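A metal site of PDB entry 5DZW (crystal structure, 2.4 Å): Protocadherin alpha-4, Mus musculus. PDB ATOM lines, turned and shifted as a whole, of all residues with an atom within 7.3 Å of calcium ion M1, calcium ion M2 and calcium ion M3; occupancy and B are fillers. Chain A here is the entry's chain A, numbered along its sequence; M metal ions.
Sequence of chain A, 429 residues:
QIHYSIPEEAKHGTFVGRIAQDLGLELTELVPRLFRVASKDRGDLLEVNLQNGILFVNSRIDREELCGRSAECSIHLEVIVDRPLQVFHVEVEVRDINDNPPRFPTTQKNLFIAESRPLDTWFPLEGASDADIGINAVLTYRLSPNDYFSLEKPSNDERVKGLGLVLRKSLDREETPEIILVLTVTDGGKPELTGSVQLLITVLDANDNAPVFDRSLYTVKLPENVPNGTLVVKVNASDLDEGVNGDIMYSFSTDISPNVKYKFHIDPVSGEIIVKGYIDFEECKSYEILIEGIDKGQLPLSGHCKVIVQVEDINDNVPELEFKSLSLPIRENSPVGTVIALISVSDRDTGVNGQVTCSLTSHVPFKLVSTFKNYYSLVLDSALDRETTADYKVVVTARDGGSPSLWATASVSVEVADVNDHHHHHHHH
Calcium ion M1 is bound by the side-chain carboxylate of Asp 239 (2.4 Å), the backbone carbonyl oxygen of Asn 209 (2.4 Å), the backbone carbonyl oxygen of Asn 245 (2.6 Å), the side-chain amide oxygen of Asn 207 (2.7 Å), the side-chain carboxylate of Asp 295 (2.8 Å) and the side-chain carboxylate of Asp 241 (2.9 Å).
Calcium ion M2 is bound by the backbone carbonyl oxygen (O) of Ala 206 (2.4 Å), the side-chain carboxylate (OD1) of Asp 205 (2.5 Å), the side-chain carboxylate (OE2) of Glu 174 (2.5 Å), the side-chain carboxylate (OD1) of Asp 241 (2.6 Å) and the side-chain carboxylate (OD1) of Asp 208 (2.8 Å).
Calcium ion M2 has five donor atoms within binding distance.
Slightly farther from calcium ion M2 lies OE1 of Glu 115 (3.1 Å).
Within 4 Å of calcium ion M2: Glu 115, Glu 174, Asp 205, Ala 206, Asp 208 and Asp 241.
OE1 of Glu 115 is in hydrogen-bond range of N of Ala 206, 3.1 Å away.
OD2 of Asp 172 is in hydrogen-bond range of N of Glu 174 (3.1 Å).
The backbone carbonyl oxygen (O) of Leu 204 sits close to the backbone NH (N) of Glu 115 (3.4 Å).
NE of Arg 173 lies close to OD1 of Asp 205, 3.6 Å away.
The backbone NH (N) of Glu 242 lies within hydrogen-bond range of the side-chain carboxylate (OD2) of Asp 205.
ND2 of Asn 207 is in hydrogen-bond range of O of Leu 299.
N of Leu 301 is in hydrogen-bond range of OD1 of Asp 295, 2.6 Å away.
The backbone NH of Glu 175 lies within hydrogen-bond range of the side-chain carboxylate of Asp 172 (2.6 Å).
Calcium ion M3 is bound by OE1 of Glu 174 (2.4 Å), OE2 of Glu 115 (2.4 Å), OD1 of Asp 208 (2.6 Å) and OD2 of Asp 208 (2.7 Å).
Slightly farther from calcium ion M3 lies the side-chain carboxylate (OD1) of Asp 172 (3.0 Å).
Within 4 Å of calcium ion M1: Asn 207, Asn 209, Asp 239, Asp 241, Asn 245 and Asp 295.
The nearest printed residue that does not touch calcium ion M1 is Ala 210 (4.6 Å).
Of the 29 residues printed, 5 come within 4 Å of calcium ion M3.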
ATOM      1  N   GLU A 115     -16.938  16.208 -29.012  1.00  0.00           N
ATOM      2  CA  GLU A 115     -15.674  16.091 -29.742  1.00  0.00           C
ATOM      3  C   GLU A 115     -15.926  15.794 -31.222  1.00  0.00           C
ATOM      4  O   GLU A 115     -15.062  16.031 -32.066  1.00  0.00           O
ATOM      5  CB  GLU A 115     -14.821  14.986 -29.120  1.00  0.00           C
ATOM      6  CG  GLU A 115     -13.422  14.852 -29.698  1.00  0.00           C
ATOM      7  CD  GLU A 115     -12.716  13.599 -29.236  1.00  0.00           C
ATOM      8  OE1 GLU A 115     -13.290  12.856 -28.411  1.00  0.00           O
ATOM      9  OE2 GLU A 115     -11.586  13.343 -29.706  1.00  0.00           O
ATOM     10  N   LEU A 171     -11.011  19.417 -32.499  1.00  0.00           N
ATOM     11  CA  LEU A 171     -10.965  19.278 -31.045  1.00  0.00           C
ATOM     12  C   LEU A 171     -10.798  17.816 -30.634  1.00  0.00           C
ATOM     13  O   LEU A 171     -11.410  16.922 -31.218  1.00  0.00           O
ATOM     14  CB  LEU A 171     -12.229  19.869 -30.415  1.00  0.00           C
ATOM     15  CG  LEU A 171     -13.573  19.145 -30.530  1.00  0.00           C
ATOM     16  CD1 LEU A 171     -14.589  19.774 -29.592  1.00  0.00           C
ATOM     17  CD2 LEU A 171     -14.111  19.147 -31.964  1.00  0.00           C
ATOM     18  N   ASP A 172      -9.971  17.584 -29.625  1.00  0.00           N
ATOM     19  CA  ASP A 172      -9.702  16.241 -29.140  1.00  0.00           C
ATOM     20  C   ASP A 172      -9.787  16.172 -27.612  1.00  0.00           C
ATOM     21  O   ASP A 172      -9.020  16.828 -26.917  1.00  0.00           O
ATOM     22  CB  ASP A 172      -8.327  15.762 -29.615  1.00  0.00           C
ATOM     23  CG  ASP A 172      -8.006  14.348 -29.154  1.00  0.00           C
ATOM     24  OD1 ASP A 172      -8.453  13.396 -29.834  1.00  0.00           O
ATOM     25  OD2 ASP A 172      -7.316  14.192 -28.130  1.00  0.00           O
ATOM     26  N   ARG A 173     -10.713  15.363 -27.121  1.00  0.00           N
ATOM     27  CA  ARG A 173     -10.954  15.217 -25.695  1.00  0.00           C
ATOM     28  C   ARG A 173      -9.719  14.700 -24.941  1.00  0.00           C
ATOM     29  O   ARG A 173      -9.430  15.160 -23.836  1.00  0.00           O
ATOM     30  CB  ARG A 173     -12.149  14.300 -25.456  1.00  0.00           C
ATOM     31  CG  ARG A 173     -12.315  13.805 -24.032  1.00  0.00           C
ATOM     32  CD  ARG A 173     -11.972  12.323 -23.926  1.00  0.00           C
ATOM     33  NE  ARG A 173     -12.360  11.760 -22.639  1.00  0.00           N
ATOM     34  CZ  ARG A 173     -11.557  11.709 -21.578  1.00  0.00           C
ATOM     35  NH1 ARG A 173     -11.985  11.177 -20.441  1.00  0.00           N
ATOM     36  NH2 ARG A 173     -10.327  12.191 -21.654  1.00  0.00           N
ATOM     37  N   GLU A 174      -9.011  13.756 -25.540  1.00  0.00           N
ATOM     38  CA  GLU A 174      -7.854  13.143 -24.905  1.00  0.00           C
ATOM     39  C   GLU A 174      -6.682  14.110 -24.749  1.00  0.00           C
ATOM     40  O   GLU A 174      -5.964  14.073 -23.761  1.00  0.00           O
ATOM     41  CB  GLU A 174      -7.399  11.898 -25.681  1.00  0.00           C
ATOM     42  CG  GLU A 174      -8.294  10.683 -25.509  1.00  0.00           C
ATOM     43  CD  GLU A 174      -9.630  10.822 -26.212  1.00  0.00           C
ATOM     44  OE1 GLU A 174      -9.733  11.660 -27.132  1.00  0.00           O
ATOM     45  OE2 GLU A 174     -10.579  10.098 -25.836  1.00  0.00           O
ATOM     46  N   GLU A 175      -6.508  14.974 -25.747  1.00  0.00           N
ATOM     47  CA  GLU A 175      -5.427  15.957 -25.708  1.00  0.00           C
ATOM     48  C   GLU A 175      -5.708  17.051 -24.675  1.00  0.00           C
ATOM     49  O   GLU A 175      -4.889  17.302 -23.786  1.00  0.00           O
ATOM     50  CB  GLU A 175      -5.223  16.580 -27.091  1.00  0.00           C
ATOM     51  CG  GLU A 175      -4.117  17.619 -27.153  1.00  0.00           C
ATOM     52  CD  GLU A 175      -3.837  18.103 -28.558  1.00  0.00           C
ATOM     53  OE1 GLU A 175      -4.129  17.341 -29.512  1.00  0.00           O
ATOM     54  OE2 GLU A 175      -3.332  19.227 -28.724  1.00  0.00           O
ATOM     55  N   LEU A 204     -16.788  16.632 -24.731  1.00  0.00           N
ATOM     56  CA  LEU A 204     -17.338  15.316 -24.453  1.00  0.00           C
ATOM     57  C   LEU A 204     -16.555  14.223 -25.178  1.00  0.00           C
ATOM     58  O   LEU A 204     -15.982  14.454 -26.240  1.00  0.00           O
ATOM     59  CB  LEU A 204     -18.816  15.268 -24.843  1.00  0.00           C
ATOM     60  CG  LEU A 204     -19.681  16.388 -24.267  1.00  0.00           C
ATOM     61  CD1 LEU A 204     -21.123  16.293 -24.750  1.00  0.00           C
ATOM     62  CD2 LEU A 204     -19.617  16.396 -22.741  1.00  0.00           C
ATOM     63  N   ASP A 205     -16.528  13.030 -24.586  1.00  0.00           N
ATOM     64  CA  ASP A 205     -15.751  11.922 -25.148  1.00  0.00           C
ATOM     65  C   ASP A 205     -16.461  11.265 -26.332  1.00  0.00           C
ATOM     66  O   ASP A 205     -17.562  10.727 -26.188  1.00  0.00           O
ATOM     67  CB  ASP A 205     -15.467  10.880 -24.069  1.00  0.00           C
ATOM     68  CG  ASP A 205     -14.640   9.714 -24.586  1.00  0.00           C
ATOM     69  OD1 ASP A 205     -13.753   9.942 -25.430  1.00  0.00           O
ATOM     70  OD2 ASP A 205     -14.879   8.571 -24.146  1.00  0.00           O
ATOM     71  N   ALA A 206     -15.828  11.320 -27.492  1.00  0.00           N
ATOM     72  CA  ALA A 206     -16.339  10.652 -28.684  1.00  0.00           C
ATOM     73  C   ALA A 206     -15.612   9.325 -28.885  1.00  0.00           C
ATOM     74  O   ALA A 206     -14.497   9.155 -28.411  1.00  0.00           O
ATOM     75  CB  ALA A 206     -16.193  11.540 -29.899  1.00  0.00           C
ATOM     76  N   ASN A 207     -16.246   8.409 -29.593  1.00  0.00           N
ATOM     77  CA  ASN A 207     -15.627   7.106 -29.866  1.00  0.00           C
ATOM     78  C   ASN A 207     -14.828   7.146 -31.170  1.00  0.00           C
ATOM     79  O   ASN A 207     -15.201   6.529 -32.160  1.00  0.00           O
ATOM     80  CB  ASN A 207     -16.687   6.007 -29.936  1.00  0.00           C
ATOM     81  CG  ASN A 207     -16.078   4.621 -29.931  1.00  0.00           C
ATOM     82  OD1 ASN A 207     -14.980   4.410 -29.424  1.00  0.00           O
ATOM     83  ND2 ASN A 207     -16.791   3.659 -30.519  1.00  0.00           N
ATOM     84  N   ASP A 208     -13.728   7.891 -31.152  1.00  0.00           N
ATOM     85  CA  ASP A 208     -12.932   8.097 -32.353  1.00  0.00           C
ATOM     86  C   ASP A 208     -11.521   7.520 -32.227  1.00  0.00           C
ATOM     87  O   ASP A 208     -10.646   7.810 -33.043  1.00  0.00           O
ATOM     88  CB  ASP A 208     -12.854   9.590 -32.692  1.00  0.00           C
ATOM     89  CG  ASP A 208     -12.324  10.422 -31.541  1.00  0.00           C
ATOM     90  OD1 ASP A 208     -12.600  10.072 -30.375  1.00  0.00           O
ATOM     91  OD2 ASP A 208     -11.633  11.431 -31.811  1.00  0.00           O
ATOM     92  N   ASN A 209     -11.301   6.698 -31.202  1.00  0.00           N
ATOM     93  CA  ASN A 209     -10.023   6.037 -31.022  1.00  0.00           C
ATOM     94  C   ASN A 209     -10.156   4.524 -30.884  1.00  0.00           C
ATOM     95  O   ASN A 209     -10.911   4.032 -30.040  1.00  0.00           O
ATOM     96  CB  ASN A 209      -9.287   6.597 -29.804  1.00  0.00           C
ATOM     97  CG  ASN A 209      -8.525   7.877 -30.116  1.00  0.00           C
ATOM     98  OD1 ASN A 209      -8.960   8.674 -30.946  1.00  0.00           O
ATOM     99  ND2 ASN A 209      -7.389   8.059 -29.460  1.00  0.00           N
ATOM    100  N   ALA A 210      -9.434   3.793 -31.726  1.00  0.00           N
ATOM    101  CA  ALA A 210      -9.459   2.332 -31.702  1.00  0.00           C
ATOM    102  C   ALA A 210      -8.482   1.794 -30.656  1.00  0.00           C
ATOM    103  O   ALA A 210      -7.464   2.422 -30.367  1.00  0.00           O
ATOM    104  CB  ALA A 210      -9.119   1.787 -33.080  1.00  0.00           C
ATOM    105  N   PRO A 211      -8.796   0.618 -30.079  1.00  0.00           N
ATOM    106  CA  PRO A 211      -7.902  -0.023 -29.123  1.00  0.00           C
ATOM    107  C   PRO A 211      -6.571  -0.425 -29.747  1.00  0.00           C
ATOM    108  O   PRO A 211      -6.521  -0.705 -30.948  1.00  0.00           O
ATOM    109  CB  PRO A 211      -8.694  -1.257 -28.674  1.00  0.00           C
ATOM    110  CG  PRO A 211      -9.702  -1.488 -29.741  1.00  0.00           C
ATOM    111  CD  PRO A 211     -10.054  -0.125 -30.253  1.00  0.00           C
ATOM    112  N   ASP A 239      -6.961   1.608 -24.757  1.00  0.00           N
ATOM    113  CA  ASP A 239      -7.771   2.523 -25.548  1.00  0.00           C
ATOM    114  C   ASP A 239      -7.937   3.860 -24.826  1.00  0.00           C
ATOM    115  O   ASP A 239      -8.186   3.898 -23.623  1.00  0.00           O
ATOM    116  CB  ASP A 239      -9.136   1.897 -25.855  1.00  0.00           C
ATOM    117  CG  ASP A 239      -9.941   2.701 -26.859  1.00  0.00           C
ATOM    118  OD1 ASP A 239      -9.354   3.588 -27.526  1.00  0.00           O
ATOM    119  OD2 ASP A 239     -11.150   2.444 -26.986  1.00  0.00           O
ATOM    120  N   LEU A 240      -7.806   4.952 -25.583  1.00  0.00           N
ATOM    121  CA  LEU A 240      -7.772   6.283 -24.992  1.00  0.00           C
ATOM    122  C   LEU A 240      -9.149   6.807 -24.587  1.00  0.00           C
ATOM    123  O   LEU A 240      -9.253   7.682 -23.735  1.00  0.00           O
ATOM    124  CB  LEU A 240      -7.112   7.262 -25.966  1.00  0.00           C
ATOM    125  CG  LEU A 240      -5.626   7.031 -26.213  1.00  0.00           C
ATOM    126  CD1 LEU A 240      -5.049   8.103 -27.125  1.00  0.00           C
ATOM    127  CD2 LEU A 240      -4.863   6.990 -24.892  1.00  0.00           C
ATOM    128  N   ASP A 241     -10.199   6.263 -25.189  1.00  0.00           N
ATOM    129  CA  ASP A 241     -11.556   6.690 -24.854  1.00  0.00           C
ATOM    130  C   ASP A 241     -11.985   6.161 -23.491  1.00  0.00           C
ATOM    131  O   ASP A 241     -11.346   5.261 -22.937  1.00  0.00           O
ATOM    132  CB  ASP A 241     -12.545   6.244 -25.938  1.00  0.00           C
ATOM    133  CG  ASP A 241     -12.224   6.821 -27.296  1.00  0.00           C
ATOM    134  OD1 ASP A 241     -11.289   7.641 -27.390  1.00  0.00           O
ATOM    135  OD2 ASP A 241     -12.917   6.473 -28.271  1.00  0.00           O
ATOM    136  N   GLU A 242     -13.060   6.722 -22.955  1.00  0.00           N
ATOM    137  CA  GLU A 242     -13.530   6.352 -21.620  1.00  0.00           C
ATOM    138  C   GLU A 242     -14.930   5.737 -21.659  1.00  0.00           C
ATOM    139  O   GLU A 242     -15.620   5.808 -22.673  1.00  0.00           O
ATOM    140  CB  GLU A 242     -13.520   7.572 -20.700  1.00  0.00           C
ATOM    141  N   VAL A 244     -17.843   2.976 -21.893  1.00  0.00           N
ATOM    142  CA  VAL A 244     -18.017   1.804 -22.728  1.00  0.00           C
ATOM    143  C   VAL A 244     -17.193   1.931 -24.009  1.00  0.00           C
ATOM    144  O   VAL A 244     -16.926   0.947 -24.691  1.00  0.00           O
ATOM    145  CB  VAL A 244     -19.495   1.570 -23.093  1.00  0.00           C
ATOM    146  CG1 VAL A 244     -20.313   1.259 -21.851  1.00  0.00           C
ATOM    147  CG2 VAL A 244     -20.070   2.780 -23.826  1.00  0.00           C
ATOM    148  N   ASN A 245     -16.793   3.165 -24.330  1.00  0.00           N
ATOM    149  CA  ASN A 245     -15.942   3.412 -25.480  1.00  0.00           C
ATOM    150  C   ASN A 245     -14.492   3.055 -25.183  1.00  0.00           C
ATOM    151  O   ASN A 245     -13.653   3.041 -26.078  1.00  0.00           O
ATOM    152  CB  ASN A 245     -16.041   4.874 -25.919  1.00  0.00           C
ATOM    153  CG  ASN A 245     -17.446   5.257 -26.357  1.00  0.00           C
ATOM    154  OD1 ASN A 245     -18.369   4.458 -26.264  1.00  0.00           O
ATOM    155  ND2 ASN A 245     -17.594   6.484 -26.825  1.00  0.00           N
ATOM    156  N   GLY A 246     -14.218   2.755 -23.919  1.00  0.00           N
ATOM    157  CA  GLY A 246     -12.875   2.404 -23.488  1.00  0.00           C
ATOM    158  C   GLY A 246     -12.705   0.925 -23.183  1.00  0.00           C
ATOM    159  O   GLY A 246     -11.622   0.365 -23.354  1.00  0.00           O
ATOM    160  N   ASP A 247     -13.782   0.284 -22.716  1.00  0.00           N
ATOM    161  CA  ASP A 247     -13.739  -1.139 -22.384  1.00  0.00           C
ATOM    162  C   ASP A 247     -13.562  -1.994 -23.632  1.00  0.00           C
ATOM    163  O   ASP A 247     -14.228  -1.775 -24.639  1.00  0.00           O
ATOM    164  CB  ASP A 247     -15.009  -1.550 -21.634  1.00  0.00           C
ATOM    165  CG  ASP A 247     -15.052  -1.017 -20.216  1.00  0.00           C
ATOM    166  OD1 ASP A 247     -14.555   0.105 -19.982  1.00  0.00           O
ATOM    167  OD2 ASP A 247     -15.583  -1.716 -19.333  1.00  0.00           O
ATOM    168  N   ILE A 248     -12.656  -2.974 -23.552  1.00  0.00           N
ATOM    169  CA  ILE A 248     -12.306  -3.786 -24.711  1.00  0.00           C
ATOM    170  C   ILE A 248     -12.662  -5.261 -24.533  1.00  0.00           C
ATOM    171  O   ILE A 248     -12.343  -5.871 -23.515  1.00  0.00           O
ATOM    172  CB  ILE A 248     -10.797  -3.680 -25.012  1.00  0.00           C
ATOM    173  CG1 ILE A 248     -10.348  -2.215 -25.028  1.00  0.00           C
ATOM    174  CG2 ILE A 248     -10.463  -4.358 -26.340  1.00  0.00           C
ATOM    175  CD1 ILE A 248      -8.855  -2.037 -25.147  1.00  0.00           C
ATOM    176  N   ASP A 295     -13.953  -2.388 -28.912  1.00  0.00           N
ATOM    177  CA  ASP A 295     -14.556  -1.639 -27.812  1.00  0.00           C
ATOM    178  C   ASP A 295     -16.066  -1.803 -27.794  1.00  0.00           C
ATOM    179  O   ASP A 295     -16.643  -2.479 -28.646  1.00  0.00           O
ATOM    180  CB  ASP A 295     -14.175  -0.150 -27.889  1.00  0.00           C
ATOM    181  CG  ASP A 295     -14.298   0.414 -29.288  1.00  0.00           C
ATOM    182  OD1 ASP A 295     -15.212  -0.006 -30.028  1.00  0.00           O
ATOM    183  OD2 ASP A 295     -13.488   1.287 -29.655  1.00  0.00           O
ATOM    184  N   LYS A 296     -16.726  -1.184 -26.816  1.00  0.00           N
ATOM    185  CA  LYS A 296     -18.163  -1.360 -26.624  1.00  0.00           C
ATOM    186  C   LYS A 296     -18.940  -0.069 -26.838  1.00  0.00           C
ATOM    187  O   LYS A 296     -19.865   0.235 -26.086  1.00  0.00           O
ATOM    188  CB  LYS A 296     -18.434  -1.911 -25.218  1.00  0.00           C
ATOM    189  CG  LYS A 296     -17.692  -3.194 -24.889  1.00  0.00           C
ATOM    190  CD  LYS A 296     -17.967  -3.642 -23.461  1.00  0.00           C
ATOM    191  N   GLY A 297     -18.570   0.688 -27.867  1.00  0.00           N
ATOM    192  CA  GLY A 297     -19.252   1.925 -28.184  1.00  0.00           C
ATOM    193  C   GLY A 297     -20.412   1.708 -29.127  1.00  0.00           C
ATOM    194  O   GLY A 297     -20.667   0.583 -29.567  1.00  0.00           O
ATOM    195  N   LEU A 299     -20.680   2.962 -32.220  1.00  0.00           N
ATOM    196  CA  LEU A 299     -19.973   2.552 -33.423  1.00  0.00           C
ATOM    197  C   LEU A 299     -18.633   1.961 -33.024  1.00  0.00           C
ATOM    198  O   LEU A 299     -17.664   2.701 -32.818  1.00  0.00           O
ATOM    199  CB  LEU A 299     -19.787   3.722 -34.389  1.00  0.00           C
ATOM    200  CG  LEU A 299     -19.076   3.390 -35.698  1.00  0.00           C
ATOM    201  CD1 LEU A 299     -19.779   2.247 -36.413  1.00  0.00           C
ATOM    202  CD2 LEU A 299     -18.976   4.613 -36.589  1.00  0.00           C
ATOM    203  N   PRO A 300     -18.570   0.629 -32.896  1.00  0.00           N
ATOM    204  CA  PRO A 300     -17.386  -0.081 -32.395  1.00  0.00           C
ATOM    205  C   PRO A 300     -16.156   0.102 -33.266  1.00  0.00           C
ATOM    206  O   PRO A 300     -16.258   0.077 -34.501  1.00  0.00           O
ATOM    207  CB  PRO A 300     -17.834  -1.543 -32.392  1.00  0.00           C
ATOM    208  CG  PRO A 300     -19.327  -1.501 -32.378  1.00  0.00           C
ATOM    209  CD  PRO A 300     -19.685  -0.294 -33.181  1.00  0.00           C
ATOM    210  N   LEU A 301     -15.005   0.284 -32.630  1.00  0.00           N
ATOM    211  CA  LEU A 301     -13.725   0.307 -33.334  1.00  0.00           C
ATOM    212  C   LEU A 301     -12.900  -0.918 -32.939  1.00  0.00           C
ATOM    213  O   LEU A 301     -12.947  -1.367 -31.790  1.00  0.00           O
ATOM    214  CB  LEU A 301     -12.955   1.588 -33.017  1.00  0.00           C
ATOM    215  CG  LEU A 301     -13.550   2.882 -33.581  1.00  0.00           C
ATOM    216  CD1 LEU A 301     -12.622   4.058 -33.320  1.00  0.00           C
ATOM    217  CD2 LEU A 301     -13.834   2.734 -35.069  1.00  0.00           C
HETATM  218 CA    CA M   1     -12.662   3.608 -28.387  1.00  0.00          CA
HETATM  219 CA    CA M   2     -12.461   9.991 -27.533  1.00  0.00          CA
HETATM  220 CA    CA M   3     -10.498  11.180 -29.393  1.00  0.00          CA
